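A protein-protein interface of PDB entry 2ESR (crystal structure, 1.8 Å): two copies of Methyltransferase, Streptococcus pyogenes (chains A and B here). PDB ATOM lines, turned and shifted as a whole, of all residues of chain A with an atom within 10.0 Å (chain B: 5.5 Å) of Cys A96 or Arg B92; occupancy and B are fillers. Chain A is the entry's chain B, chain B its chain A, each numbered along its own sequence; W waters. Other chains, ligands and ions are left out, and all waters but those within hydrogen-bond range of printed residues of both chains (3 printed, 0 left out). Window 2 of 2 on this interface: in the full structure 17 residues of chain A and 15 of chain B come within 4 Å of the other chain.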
ATOM      1  N   ARG A  34       0.839 -23.035 -43.082  1.00  0.00           N
ATOM      2  CA  ARG A  34       0.813 -23.302 -41.649  1.00  0.00           C
ATOM      3  C   ARG A  34      -0.074 -22.315 -40.905  1.00  0.00           C
ATOM      4  O   ARG A  34      -0.028 -21.109 -41.149  1.00  0.00           O
ATOM      5  CB  ARG A  34       2.218 -23.226 -41.061  1.00  0.00           C
ATOM      6  CG  ARG A  34       3.208 -24.202 -41.655  1.00  0.00           C
ATOM      7  CD  ARG A  34       4.473 -24.205 -40.815  1.00  0.00           C
ATOM      8  NE  ARG A  34       4.238 -24.804 -39.504  1.00  0.00           N
ATOM      9  CZ  ARG A  34       5.006 -24.599 -38.437  1.00  0.00           C
ATOM     10  NH1 ARG A  34       6.062 -23.800 -38.519  1.00  0.00           N
ATOM     11  NH2 ARG A  34       4.726 -25.206 -37.291  1.00  0.00           N
ATOM     12  N   LEU A  36      -1.542 -20.852 -37.097  1.00  0.00           N
ATOM     13  CA  LEU A  36      -1.244 -20.698 -35.683  1.00  0.00           C
ATOM     14  C   LEU A  36      -2.524 -20.198 -35.029  1.00  0.00           C
ATOM     15  O   LEU A  36      -3.044 -19.144 -35.397  1.00  0.00           O
ATOM     16  CB  LEU A  36      -0.126 -19.680 -35.441  1.00  0.00           C
ATOM     17  CG  LEU A  36       0.041 -19.264 -33.970  1.00  0.00           C
ATOM     18  CD1 LEU A  36       0.528 -20.448 -33.148  1.00  0.00           C
ATOM     19  CD2 LEU A  36       1.012 -18.104 -33.867  1.00  0.00           C
ATOM     20  N   LEU A  38      -3.484 -19.087 -31.597  1.00  0.00           N
ATOM     21  CA  LEU A  38      -2.936 -18.705 -30.290  1.00  0.00           C
ATOM     22  C   LEU A  38      -3.803 -18.897 -29.055  1.00  0.00           C
ATOM     23  O   LEU A  38      -3.276 -18.999 -27.941  1.00  0.00           O
ATOM     24  CB  LEU A  38      -2.436 -17.259 -30.328  1.00  0.00           C
ATOM     25  CG  LEU A  38      -0.956 -17.043 -30.673  1.00  0.00           C
ATOM     26  CD1 LEU A  38      -0.605 -15.567 -30.493  1.00  0.00           C
ATOM     27  CD2 LEU A  38      -0.080 -17.898 -29.759  1.00  0.00           C
ATOM     28  N   VAL A  58      -0.760 -25.235 -35.535  1.00  0.00           N
ATOM     29  CA  VAL A  58      -0.218 -25.272 -34.186  1.00  0.00           C
ATOM     30  C   VAL A  58      -1.280 -24.577 -33.351  1.00  0.00           C
ATOM     31  O   VAL A  58      -1.641 -23.427 -33.621  1.00  0.00           O
ATOM     32  CB  VAL A  58       1.110 -24.499 -34.065  1.00  0.00           C
ATOM     33  CG1 VAL A  58       1.521 -24.399 -32.601  1.00  0.00           C
ATOM     34  CG2 VAL A  58       2.194 -25.206 -34.870  1.00  0.00           C
ATOM     35  N   VAL A  60      -2.551 -23.339 -29.562  1.00  0.00           N
ATOM     36  CA  VAL A  60      -2.066 -22.968 -28.246  1.00  0.00           C
ATOM     37  C   VAL A  60      -3.278 -22.751 -27.341  1.00  0.00           C
ATOM     38  O   VAL A  60      -4.146 -21.929 -27.630  1.00  0.00           O
ATOM     39  CB  VAL A  60      -1.222 -21.681 -28.312  1.00  0.00           C
ATOM     40  CG1 VAL A  60      -0.720 -21.313 -26.922  1.00  0.00           C
ATOM     41  CG2 VAL A  60      -0.046 -21.886 -29.264  1.00  0.00           C
ATOM     42  N   LYS A  62      -4.018 -23.250 -22.931  1.00  0.00           N
ATOM     43  CA  LYS A  62      -3.598 -23.753 -21.629  1.00  0.00           C
ATOM     44  C   LYS A  62      -4.768 -24.238 -20.773  1.00  0.00           C
ATOM     45  O   LYS A  62      -4.567 -24.931 -19.779  1.00  0.00           O
ATOM     46  CB  LYS A  62      -2.815 -22.672 -20.876  1.00  0.00           C
ATOM     47  CG  LYS A  62      -2.004 -23.197 -19.696  1.00  0.00           C
ATOM     48  CD  LYS A  62      -1.288 -22.071 -18.970  1.00  0.00           C
ATOM     49  CE  LYS A  62      -0.342 -22.602 -17.900  1.00  0.00           C
ATOM     50  NZ  LYS A  62       0.801 -23.351 -18.491  1.00  0.00           N
ATOM     51  N   LEU A  86      -0.207 -27.212 -28.098  1.00  0.00           N
ATOM     52  CA  LEU A  86       0.749 -26.774 -27.091  1.00  0.00           C
ATOM     53  C   LEU A  86      -0.011 -26.164 -25.920  1.00  0.00           C
ATOM     54  O   LEU A  86      -0.823 -25.256 -26.094  1.00  0.00           O
ATOM     55  CB  LEU A  86       1.716 -25.741 -27.668  1.00  0.00           C
ATOM     56  CG  LEU A  86       2.626 -26.230 -28.798  1.00  0.00           C
ATOM     57  CD1 LEU A  86       3.527 -25.085 -29.237  1.00  0.00           C
ATOM     58  CD2 LEU A  86       3.451 -27.424 -28.331  1.00  0.00           C
ATOM     59  N   LYS A  87       0.261 -26.679 -24.730  1.00  0.00           N
ATOM     60  CA  LYS A  87      -0.388 -26.221 -23.509  1.00  0.00           C
ATOM     61  C   LYS A  87       0.486 -25.167 -22.838  1.00  0.00           C
ATOM     62  O   LYS A  87       1.283 -25.470 -21.950  1.00  0.00           O
ATOM     63  CB  LYS A  87      -0.602 -27.426 -22.588  1.00  0.00           C
ATOM     64  CG  LYS A  87      -1.098 -27.121 -21.187  1.00  0.00           C
ATOM     65  CD  LYS A  87      -1.287 -28.430 -20.422  1.00  0.00           C
ATOM     66  CE  LYS A  87      -0.016 -29.276 -20.463  1.00  0.00           C
ATOM     67  NZ  LYS A  87      -0.266 -30.694 -20.087  1.00  0.00           N
ATOM     68  N   MET A  88       0.340 -23.921 -23.272  1.00  0.00           N
ATOM     69  CA  MET A  88       1.141 -22.840 -22.720  1.00  0.00           C
ATOM     70  C   MET A  88       0.488 -21.486 -22.969  1.00  0.00           C
ATOM     71  O   MET A  88      -0.466 -21.381 -23.741  1.00  0.00           O
ATOM     72  CB  MET A  88       2.553 -22.885 -23.337  1.00  0.00           C
ATOM     73  CG  MET A  88       2.601 -22.714 -24.853  1.00  0.00           C
ATOM     74  SD  MET A  88       4.307 -23.240 -25.697  1.00  0.00           S
ATOM     75  CE  MET A  88       5.494 -22.099 -24.714  1.00  0.00           C
ATOM     76  N   GLU A  89       0.992 -20.459 -22.290  1.00  0.00           N
ATOM     77  CA  GLU A  89       0.483 -19.101 -22.445  1.00  0.00           C
ATOM     78  C   GLU A  89       0.838 -18.612 -23.843  1.00  0.00           C
ATOM     79  O   GLU A  89       1.868 -18.995 -24.391  1.00  0.00           O
ATOM     80  CB  GLU A  89       1.118 -18.178 -21.401  1.00  0.00           C
ATOM     81  CG  GLU A  89       0.499 -18.279 -20.019  1.00  0.00           C
ATOM     82  CD  GLU A  89      -0.893 -17.671 -19.962  1.00  0.00           C
ATOM     83  OE1 GLU A  89      -1.031 -16.472 -20.287  1.00  0.00           O
ATOM     84  OE2 GLU A  89      -1.848 -18.387 -19.593  1.00  0.00           O
ATOM     85  N   ALA A  90      -0.013 -17.770 -24.417  1.00  0.00           N
ATOM     86  CA  ALA A  90       0.242 -17.252 -25.754  1.00  0.00           C
ATOM     87  C   ALA A  90       1.583 -16.524 -25.834  1.00  0.00           C
ATOM     88  O   ALA A  90       2.345 -16.737 -26.771  1.00  0.00           O
ATOM     89  CB  ALA A  90      -0.891 -16.322 -26.184  1.00  0.00           C
ATOM     90  N   GLU A  91       1.870 -15.677 -24.848  1.00  0.00           N
ATOM     91  CA  GLU A  91       3.121 -14.917 -24.827  1.00  0.00           C
ATOM     92  C   GLU A  91       4.323 -15.863 -24.854  1.00  0.00           C
ATOM     93  O   GLU A  91       5.305 -15.625 -25.560  1.00  0.00           O
ATOM     94  CB  GLU A  91       3.203 -14.042 -23.570  1.00  0.00           C
ATOM     95  CG  GLU A  91       1.968 -13.198 -23.275  1.00  0.00           C
ATOM     96  CD  GLU A  91       0.936 -13.931 -22.430  1.00  0.00           C
ATOM     97  OE1 GLU A  91       0.213 -14.794 -22.970  1.00  0.00           O
ATOM     98  OE2 GLU A  91       0.857 -13.646 -21.214  1.00  0.00           O
ATOM     99  N   ARG A  92       4.227 -16.937 -24.078  1.00  0.00           N
ATOM    100  CA  ARG A  92       5.283 -17.939 -23.994  1.00  0.00           C
ATOM    101  C   ARG A  92       5.449 -18.605 -25.362  1.00  0.00           C
ATOM    102  O   ARG A  92       6.564 -18.754 -25.863  1.00  0.00           O
ATOM    103  CB  ARG A  92       4.906 -18.987 -22.944  1.00  0.00           C
ATOM    104  CG  ARG A  92       6.073 -19.664 -22.245  1.00  0.00           C
ATOM    105  CD  ARG A  92       5.586 -20.879 -21.458  1.00  0.00           C
ATOM    106  NE  ARG A  92       4.314 -20.620 -20.784  1.00  0.00           N
ATOM    107  CZ  ARG A  92       3.631 -21.528 -20.098  1.00  0.00           C
ATOM    108  NH1 ARG A  92       4.093 -22.766 -19.986  1.00  0.00           N
ATOM    109  NH2 ARG A  92       2.490 -21.203 -19.529  1.00  0.00           N
ATOM    110  N   ALA A  93       4.331 -19.001 -25.964  1.00  0.00           N
ATOM    111  CA  ALA A  93       4.358 -19.650 -27.271  1.00  0.00           C
ATOM    112  C   ALA A  93       5.060 -18.789 -28.306  1.00  0.00           C
ATOM    113  O   ALA A  93       5.846 -19.284 -29.111  1.00  0.00           O
ATOM    114  CB  ALA A  93       2.940 -19.956 -27.731  1.00  0.00           C
ATOM    115  N   ILE A  94       4.776 -17.491 -28.291  1.00  0.00           N
ATOM    116  CA  ILE A  94       5.392 -16.598 -29.257  1.00  0.00           C
ATOM    117  C   ILE A  94       6.913 -16.544 -29.105  1.00  0.00           C
ATOM    118  O   ILE A  94       7.637 -16.369 -30.085  1.00  0.00           O
ATOM    119  CB  ILE A  94       4.789 -15.185 -29.144  1.00  0.00           C
ATOM    120  CG1 ILE A  94       3.313 -15.249 -29.535  1.00  0.00           C
ATOM    121  CG2 ILE A  94       5.523 -14.220 -30.056  1.00  0.00           C
ATOM    122  CD1 ILE A  94       2.546 -13.963 -29.301  1.00  0.00           C
ATOM    123  N   ASP A  95       7.395 -16.710 -27.879  1.00  0.00           N
ATOM    124  CA  ASP A  95       8.832 -16.678 -27.626  1.00  0.00           C
ATOM    125  C   ASP A  95       9.521 -18.010 -27.888  1.00  0.00           C
ATOM    126  O   ASP A  95      10.749 -18.075 -27.891  1.00  0.00           O
ATOM    127  CB  ASP A  95       9.106 -16.254 -26.180  1.00  0.00           C
ATOM    128  CG  ASP A  95       9.006 -14.751 -25.981  1.00  0.00           C
ATOM    129  OD1 ASP A  95       8.972 -14.308 -24.813  1.00  0.00           O
ATOM    130  OD2 ASP A  95       8.976 -14.010 -26.987  1.00  0.00           O
ATOM    131  N   CYS A  96       8.751 -19.069 -28.118  1.00  0.00           N
ATOM    132  CA  CYS A  96       9.356 -20.380 -28.342  1.00  0.00           C
ATOM    133  C   CYS A  96       9.189 -20.939 -29.750  1.00  0.00           C
ATOM    134  O   CYS A  96      10.010 -21.741 -30.208  1.00  0.00           O
ATOM    135  CB  CYS A  96       8.802 -21.386 -27.334  1.00  0.00           C
ATOM    136  SG  CYS A  96       9.131 -20.953 -25.599  1.00  0.00           S
ATOM    137  N   LEU A  97       8.125 -20.535 -30.436  1.00  0.00           N
ATOM    138  CA  LEU A  97       7.886 -21.024 -31.789  1.00  0.00           C
ATOM    139  C   LEU A  97       8.877 -20.424 -32.783  1.00  0.00           C
ATOM    140  O   LEU A  97       9.392 -19.327 -32.585  1.00  0.00           O
ATOM    141  CB  LEU A  97       6.447 -20.704 -32.216  1.00  0.00           C
ATOM    142  CG  LEU A  97       5.368 -21.537 -31.518  1.00  0.00           C
ATOM    143  CD1 LEU A  97       3.993 -20.997 -31.846  1.00  0.00           C
ATOM    144  CD2 LEU A  97       5.490 -22.990 -31.955  1.00  0.00           C
ATOM    145  N   THR A  98       9.158 -21.162 -33.849  1.00  0.00           N
ATOM    146  CA  THR A  98      10.072 -20.686 -34.877  1.00  0.00           C
ATOM    147  C   THR A  98       9.390 -20.896 -36.221  1.00  0.00           C
ATOM    148  O   THR A  98       8.215 -21.259 -36.274  1.00  0.00           O
ATOM    149  CB  THR A  98      11.404 -21.463 -34.854  1.00  0.00           C
ATOM    150  OG1 THR A  98      11.163 -22.833 -35.186  1.00  0.00           O
ATOM    151  CG2 THR A  98      12.042 -21.386 -33.478  1.00  0.00           C
ATOM    152  N   GLY A  99      10.117 -20.676 -37.309  1.00  0.00           N
ATOM    153  CA  GLY A  99       9.510 -20.851 -38.614  1.00  0.00           C
ATOM    154  C   GLY A  99       8.465 -19.772 -38.825  1.00  0.00           C
ATOM    155  O   GLY A  99       8.321 -18.877 -37.990  1.00  0.00           O
ATOM    156  N   PHE A 101       4.329 -18.540 -40.071  1.00  0.00           N
ATOM    157  CA  PHE A 101       2.928 -18.904 -40.196  1.00  0.00           C
ATOM    158  C   PHE A 101       2.233 -18.081 -41.270  1.00  0.00           C
ATOM    159  O   PHE A 101       2.455 -16.875 -41.384  1.00  0.00           O
ATOM    160  CB  PHE A 101       2.241 -18.722 -38.843  1.00  0.00           C
ATOM    161  CG  PHE A 101       2.646 -19.749 -37.829  1.00  0.00           C
ATOM    162  CD1 PHE A 101       2.105 -21.035 -37.874  1.00  0.00           C
ATOM    163  CD2 PHE A 101       3.596 -19.452 -36.857  1.00  0.00           C
ATOM    164  CE1 PHE A 101       2.504 -22.007 -36.969  1.00  0.00           C
ATOM    165  CE2 PHE A 101       4.006 -20.422 -35.942  1.00  0.00           C
ATOM    166  CZ  PHE A 101       3.460 -21.700 -35.997  1.00  0.00           C
ATOM    167  N   ALA A 121       4.557  -8.499 -31.583  1.00  0.00           N
ATOM    168  CA  ALA A 121       5.440  -9.550 -31.078  1.00  0.00           C
ATOM    169  C   ALA A 121       5.664 -10.617 -32.155  1.00  0.00           C
ATOM    170  O   ALA A 121       6.785 -11.068 -32.373  1.00  0.00           O
ATOM    171  CB  ALA A 121       4.828 -10.184 -29.836  1.00  0.00           C
ATOM    172  N   LEU A 122       4.591 -11.023 -32.824  1.00  0.00           N
ATOM    173  CA  LEU A 122       4.694 -12.031 -33.875  1.00  0.00           C
ATOM    174  C   LEU A 122       5.621 -11.535 -34.978  1.00  0.00           C
ATOM    175  O   LEU A 122       6.485 -12.277 -35.458  1.00  0.00           O
ATOM    176  CB  LEU A 122       3.308 -12.332 -34.457  1.00  0.00           C
ATOM    177  CG  LEU A 122       2.375 -13.136 -33.551  1.00  0.00           C
ATOM    178  CD1 LEU A 122       0.951 -13.047 -34.065  1.00  0.00           C
ATOM    179  CD2 LEU A 122       2.834 -14.582 -33.495  1.00  0.00           C
ATOM    180  N   LYS A 125       9.265 -11.408 -33.792  1.00  0.00           N
ATOM    181  CA  LYS A 125       9.861 -12.732 -33.647  1.00  0.00           C
ATOM    182  C   LYS A 125       9.938 -13.472 -34.983  1.00  0.00           C
ATOM    183  O   LYS A 125      10.236 -14.667 -35.021  1.00  0.00           O
ATOM    184  CB  LYS A 125       9.061 -13.569 -32.642  1.00  0.00           C
ATOM    185  CG  LYS A 125       9.081 -13.030 -31.219  1.00  0.00           C
ATOM    186  CD  LYS A 125      10.471 -13.124 -30.613  1.00  0.00           C
ATOM    187  CE  LYS A 125      10.508 -12.535 -29.211  1.00  0.00           C
ATOM    188  NZ  LYS A 125      11.880 -12.599 -28.626  1.00  0.00           N
ATOM    189  N   LEU A 127       7.708 -14.595 -36.977  1.00  0.00           N
ATOM    190  CA  LEU A 127       6.839 -15.761 -37.033  1.00  0.00           C
ATOM    191  C   LEU A 127       5.787 -15.681 -38.131  1.00  0.00           C
ATOM    192  O   LEU A 127       5.015 -16.622 -38.324  1.00  0.00           O
ATOM    193  CB  LEU A 127       6.146 -15.958 -35.686  1.00  0.00           C
ATOM    194  CG  LEU A 127       7.070 -16.333 -34.527  1.00  0.00           C
ATOM    195  CD1 LEU A 127       6.262 -16.442 -33.246  1.00  0.00           C
ATOM    196  CD2 LEU A 127       7.776 -17.649 -34.841  1.00  0.00           C
ATOM    197  N   LYS B  62      17.511 -25.680 -28.092  1.00  0.00           N
ATOM    198  CA  LYS B  62      17.761 -24.373 -27.488  1.00  0.00           C
ATOM    199  C   LYS B  62      18.858 -23.525 -28.132  1.00  0.00           C
ATOM    200  O   LYS B  62      18.807 -22.295 -28.068  1.00  0.00           O
ATOM    201  CB  LYS B  62      18.074 -24.545 -26.000  1.00  0.00           C
ATOM    202  CG  LYS B  62      17.038 -23.931 -25.072  1.00  0.00           C
ATOM    203  CD  LYS B  62      16.828 -22.451 -25.377  1.00  0.00           C
ATOM    204  CE  LYS B  62      15.779 -21.838 -24.468  1.00  0.00           C
ATOM    205  NZ  LYS B  62      15.458 -20.445 -24.872  1.00  0.00           N
ATOM    206  N   LEU B  85       9.230 -26.475 -34.780  1.00  0.00           N
ATOM    207  CA  LEU B  85      10.461 -26.281 -34.024  1.00  0.00           C
ATOM    208  C   LEU B  85      10.215 -25.375 -32.826  1.00  0.00           C
ATOM    209  O   LEU B  85       9.672 -24.277 -32.959  1.00  0.00           O
ATOM    210  CB  LEU B  85      11.561 -25.666 -34.902  1.00  0.00           C
ATOM    211  CG  LEU B  85      12.858 -25.309 -34.157  1.00  0.00           C
ATOM    212  CD1 LEU B  85      13.537 -26.583 -33.671  1.00  0.00           C
ATOM    213  CD2 LEU B  85      13.802 -24.533 -35.063  1.00  0.00           C
ATOM    214  N   LEU B  86      10.612 -25.849 -31.654  1.00  0.00           N
ATOM    215  CA  LEU B  86      10.451 -25.086 -30.428  1.00  0.00           C
ATOM    216  C   LEU B  86      11.828 -24.728 -29.901  1.00  0.00           C
ATOM    217  O   LEU B  86      12.693 -25.595 -29.755  1.00  0.00           O
ATOM    218  CB  LEU B  86       9.699 -25.907 -29.380  1.00  0.00           C
ATOM    219  CG  LEU B  86       8.252 -26.287 -29.707  1.00  0.00           C
ATOM    220  CD1 LEU B  86       7.704 -27.191 -28.617  1.00  0.00           C
ATOM    221  CD2 LEU B  86       7.409 -25.030 -29.832  1.00  0.00           C
ATOM    222  N   LYS B  87      12.030 -23.444 -29.629  1.00  0.00           N
ATOM    223  CA  LYS B  87      13.293 -22.960 -29.096  1.00  0.00           C
ATOM    224  C   LYS B  87      13.102 -22.850 -27.592  1.00  0.00           C
ATOM    225  O   LYS B  87      12.684 -21.809 -27.079  1.00  0.00           O
ATOM    226  CB  LYS B  87      13.638 -21.596 -29.696  1.00  0.00           C
ATOM    227  CG  LYS B  87      15.010 -21.075 -29.297  1.00  0.00           C
ATOM    228  CD  LYS B  87      15.534 -20.040 -30.291  1.00  0.00           C
ATOM    229  CE  LYS B  87      14.587 -18.857 -30.443  1.00  0.00           C
ATOM    230  NZ  LYS B  87      15.077 -17.889 -31.472  1.00  0.00           N
ATOM    231  N   MET B  88      13.387 -23.936 -26.886  1.00  0.00           N
ATOM    232  CA  MET B  88      13.221 -23.945 -25.441  1.00  0.00           C
ATOM    233  C   MET B  88      13.940 -25.127 -24.804  1.00  0.00           C
ATOM    234  O   MET B  88      14.448 -26.010 -25.500  1.00  0.00           O
ATOM    235  CB  MET B  88      11.721 -23.968 -25.089  1.00  0.00           C
ATOM    236  CG  MET B  88      10.955 -25.194 -25.571  1.00  0.00           C
ATOM    237  SD  MET B  88       9.008 -24.964 -25.558  1.00  0.00           S
ATOM    238  CE  MET B  88       8.747 -24.749 -23.651  1.00  0.00           C
ATOM    239  N   GLU B  89      14.006 -25.126 -23.477  1.00  0.00           N
ATOM    240  CA  GLU B  89      14.651 -26.204 -22.739  1.00  0.00           C
ATOM    241  C   GLU B  89      13.779 -27.450 -22.853  1.00  0.00           C
ATOM    242  O   GLU B  89      12.553 -27.358 -22.820  1.00  0.00           O
ATOM    243  CB  GLU B  89      14.797 -25.829 -21.261  1.00  0.00           C
ATOM    244  CG  GLU B  89      15.553 -24.531 -20.993  1.00  0.00           C
ATOM    245  CD  GLU B  89      17.000 -24.583 -21.436  1.00  0.00           C
ATOM    246  OE1 GLU B  89      17.743 -23.622 -21.140  1.00  0.00           O
ATOM    247  OE2 GLU B  89      17.396 -25.576 -22.081  1.00  0.00           O
ATOM    248  N   ALA B  90      14.409 -28.611 -22.985  1.00  0.00           N
ATOM    249  CA  ALA B  90      13.669 -29.866 -23.108  1.00  0.00           C
ATOM    250  C   ALA B  90      12.685 -30.050 -21.957  1.00  0.00           C
ATOM    251  O   ALA B  90      11.551 -30.482 -22.162  1.00  0.00           O
ATOM    252  CB  ALA B  90      14.638 -31.036 -23.157  1.00  0.00           C
ATOM    253  N   GLU B  91      13.128 -29.719 -20.748  1.00  0.00           N
ATOM    254  CA  GLU B  91      12.299 -29.837 -19.555  1.00  0.00           C
ATOM    255  C   GLU B  91      11.045 -28.977 -19.660  1.00  0.00           C
ATOM    256  O   GLU B  91       9.939 -29.428 -19.344  1.00  0.00           O
ATOM    257  CB  GLU B  91      13.115 -29.435 -18.325  1.00  0.00           C
ATOM    258  CG  GLU B  91      14.157 -30.471 -17.924  1.00  0.00           C
ATOM    259  CD  GLU B  91      15.293 -29.890 -17.099  1.00  0.00           C
ATOM    260  OE1 GLU B  91      15.022 -29.116 -16.158  1.00  0.00           O
ATOM    261  OE2 GLU B  91      16.463 -30.221 -17.393  1.00  0.00           O
ATOM    262  N   ARG B  92      11.220 -27.736 -20.103  1.00  0.00           N
ATOM    263  CA  ARG B  92      10.097 -26.820 -20.263  1.00  0.00           C
ATOM    264  C   ARG B  92       9.180 -27.353 -21.356  1.00  0.00           C
ATOM    265  O   ARG B  92       7.958 -27.357 -21.211  1.00  0.00           O
ATOM    266  CB  ARG B  92      10.601 -25.431 -20.666  1.00  0.00           C
ATOM    267  CG  ARG B  92      11.406 -24.702 -19.609  1.00  0.00           C
ATOM    268  CD  ARG B  92      12.419 -23.767 -20.263  1.00  0.00           C
ATOM    269  NE  ARG B  92      11.839 -22.958 -21.336  1.00  0.00           N
ATOM    270  CZ  ARG B  92      12.550 -22.277 -22.226  1.00  0.00           C
ATOM    271  NH1 ARG B  92      13.870 -22.306 -22.183  1.00  0.00           N
ATOM    272  NH2 ARG B  92      11.942 -21.558 -23.155  1.00  0.00           N
ATOM    273  N   ALA B  93       9.786 -27.799 -22.453  1.00  0.00           N
ATOM    274  CA  ALA B  93       9.037 -28.330 -23.584  1.00  0.00           C
ATOM    275  C   ALA B  93       8.110 -29.463 -23.166  1.00  0.00           C
ATOM    276  O   ALA B  93       6.924 -29.443 -23.481  1.00  0.00           O
ATOM    277  CB  ALA B  93      10.003 -28.808 -24.680  1.00  0.00           C
ATOM    278  N   ILE B  94       8.647 -30.445 -22.446  1.00  0.00           N
ATOM    279  CA  ILE B  94       7.847 -31.580 -22.008  1.00  0.00           C
ATOM    280  C   ILE B  94       6.581 -31.164 -21.255  1.00  0.00           C
ATOM    281  O   ILE B  94       5.545 -31.816 -21.368  1.00  0.00           O
ATOM    282  CB  ILE B  94       8.701 -32.545 -21.142  1.00  0.00           C
ATOM    283  CG1 ILE B  94       9.785 -33.178 -22.021  1.00  0.00           C
ATOM    284  CG2 ILE B  94       7.820 -33.633 -20.529  1.00  0.00           C
ATOM    285  CD1 ILE B  94      10.776 -34.047 -21.263  1.00  0.00           C
ATOM    286  N   ASP B  95       6.654 -30.070 -20.504  1.00  0.00           N
ATOM    287  CA  ASP B  95       5.494 -29.594 -19.754  1.00  0.00           C
ATOM    288  C   ASP B  95       4.440 -28.923 -20.634  1.00  0.00           C
ATOM    289  O   ASP B  95       3.300 -28.733 -20.210  1.00  0.00           O
ATOM    290  CB  ASP B  95       5.940 -28.615 -18.663  1.00  0.00           C
ATOM    291  CG  ASP B  95       6.665 -29.305 -17.524  1.00  0.00           C
ATOM    292  OD1 ASP B  95       6.063 -30.211 -16.908  1.00  0.00           O
ATOM    293  OD2 ASP B  95       7.829 -28.944 -17.241  1.00  0.00           O
ATOM    294  N   CYS B  96       4.815 -28.574 -21.859  1.00  0.00           N
ATOM    295  CA  CYS B  96       3.895 -27.905 -22.769  1.00  0.00           C
ATOM    296  C   CYS B  96       3.343 -28.810 -23.870  1.00  0.00           C
ATOM    297  O   CYS B  96       2.374 -28.457 -24.541  1.00  0.00           O
ATOM    298  CB  CYS B  96       4.587 -26.695 -23.394  1.00  0.00           C
ATOM    299  SG  CYS B  96       5.165 -25.490 -22.176  1.00  0.00           S
HETATM  300  O   HOH W   1       8.630 -24.757 -36.987  1.00  0.00           O
HETATM  301  O   HOH W   2       9.569 -21.018 -21.890  1.00  0.00           O
HETATM  302  O   HOH W   3       2.583 -25.427 -19.469  1.00  0.00           O
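The backbone carbonyl oxygen (O) of Leu B85 lies close to the side-chain hydroxyl (OG1) of Thr A98. The backbone NH (N) of Lys B87 lies within hydrogen-bond range of the backbone carbonyl oxygen (O) of Cys A96, 2.7 Å away. The guanidinium group of Arg B92 sits at hydrogen-bond distance from the side-chain sulfur of Cys A96 (3.8 Å). The backbone carbonyl oxygen (O) of Cys B96 lies within hydrogen-bond range of the backbone NH (N) of Lys A87, 2.8 Å away. The side-chain sulfur of Cys B96 lies within hydrogen-bond range of the guanidinium group of Arg A92.
The side-chain sulfur (SG) of Cys B96 lies within hydrogen-bond range of the backbone carbonyl oxygen (O) of Arg B92 (3.5 Å). The backbone carbonyl oxygen (O) of Arg A92 lies within hydrogen-bond range of the side-chain sulfur (SG) of Cys A96 (3.4 Å).
Leu A86 touches Leu B86. Leu A86 touches Cys B96. Lys A87 touches Asp B95 (CE to O, 3.4 Å). Met A88 touches Cys B96 (CB to SG, 3.9 Å). Cys A96 touches Leu B85. Cys A96 touches Leu B86 (O to CA, 3.4 Å). CB of Cys A96 touches SD of Met B88, 3.9998 Å away. O of Leu B85 touches CA of Leu A97 (3.9 Å). Leu B86 touches Leu A97.
Printed residues of chain B within 4 Å of Cys A96: Leu B85 (3.8 Å), Leu B86 (3.4 Å), Lys B87 (2.7 Å), Met B88 (3.9998 Å) and Arg B92 (3.8 Å). Arg B92 touches one residue of chain A. Glu B89 touches none of the printed residues of chain A. Asp B95 touches just one residue of chain A: Lys A87. Printed residues of chain B within 4 Å of Thr A98: Leu B85. Of the printed residues of chain B, Leu A86 touches Leu B86 (3.9 Å) and Cys B96 (3.5 Å). Printed residues of chain A within 4 Å of Lys B87: Cys A96 (2.7 Å). Printed residues of chain B within 4 Å of Lys A87: Asp B95 and Cys B96. Gly A99 touches none of the printed residues of chain B. Glu A91 touches none of the printed residues of chain B. The nearest printed residue of chain B that does not touch Cys A96 is Lys B62 (6.4 Å).
Printed residues of chain B that touch a printed residue of chain A: Leu B85, Leu B86, Lys B87, Met B88, Arg B92, Asp B95 and Cys B96. Hydrophobic or aromatic side chains of chain B that line the printed part of chain A: Leu B85, Leu B86 and Met B88. Of the 25 printed residues of chain A, 7 touch a printed residue of chain B. Hydrophobic or aromatic side chains of chain A within 4 Å of the printed part of chain B: Leu A86, Met A88 and Leu A97. Among the printed residues, no Asp or Glu carboxylate lies within 4 Å of a Lys or Arg side-chain nitrogen of the other chain.
Leu A86 touches Cys B96, and with the chains exchanged Cys A96 touches Leu B86. Lys A87 touches Asp B95, but with the chains exchanged Asp A95 does not touch Lys B87 (4.3 Å). Met A88 touches Cys B96, and with the chains exchanged Cys A96 touches Met B88. Arg A92 touches Cys B96, and with the chains exchanged Cys A96 touches Arg B92.
Water W2 lies within hydrogen-bond range of NH2 of Arg B92 (2.7 Å) and SG of Cys A96 (3.7 Å). Water W3 lies within hydrogen-bond range of O of Lys A87 (2.8 Å), NZ of Lys A62 (2.9 Å), NH1 of Arg A92 (3.1 Å), O of Asp B95 (3.5 Å) and SG of Cys B96 (3.7 Å). Water W1 lies within hydrogen-bond range of N of Leu B85 and NH1 of Arg A34.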
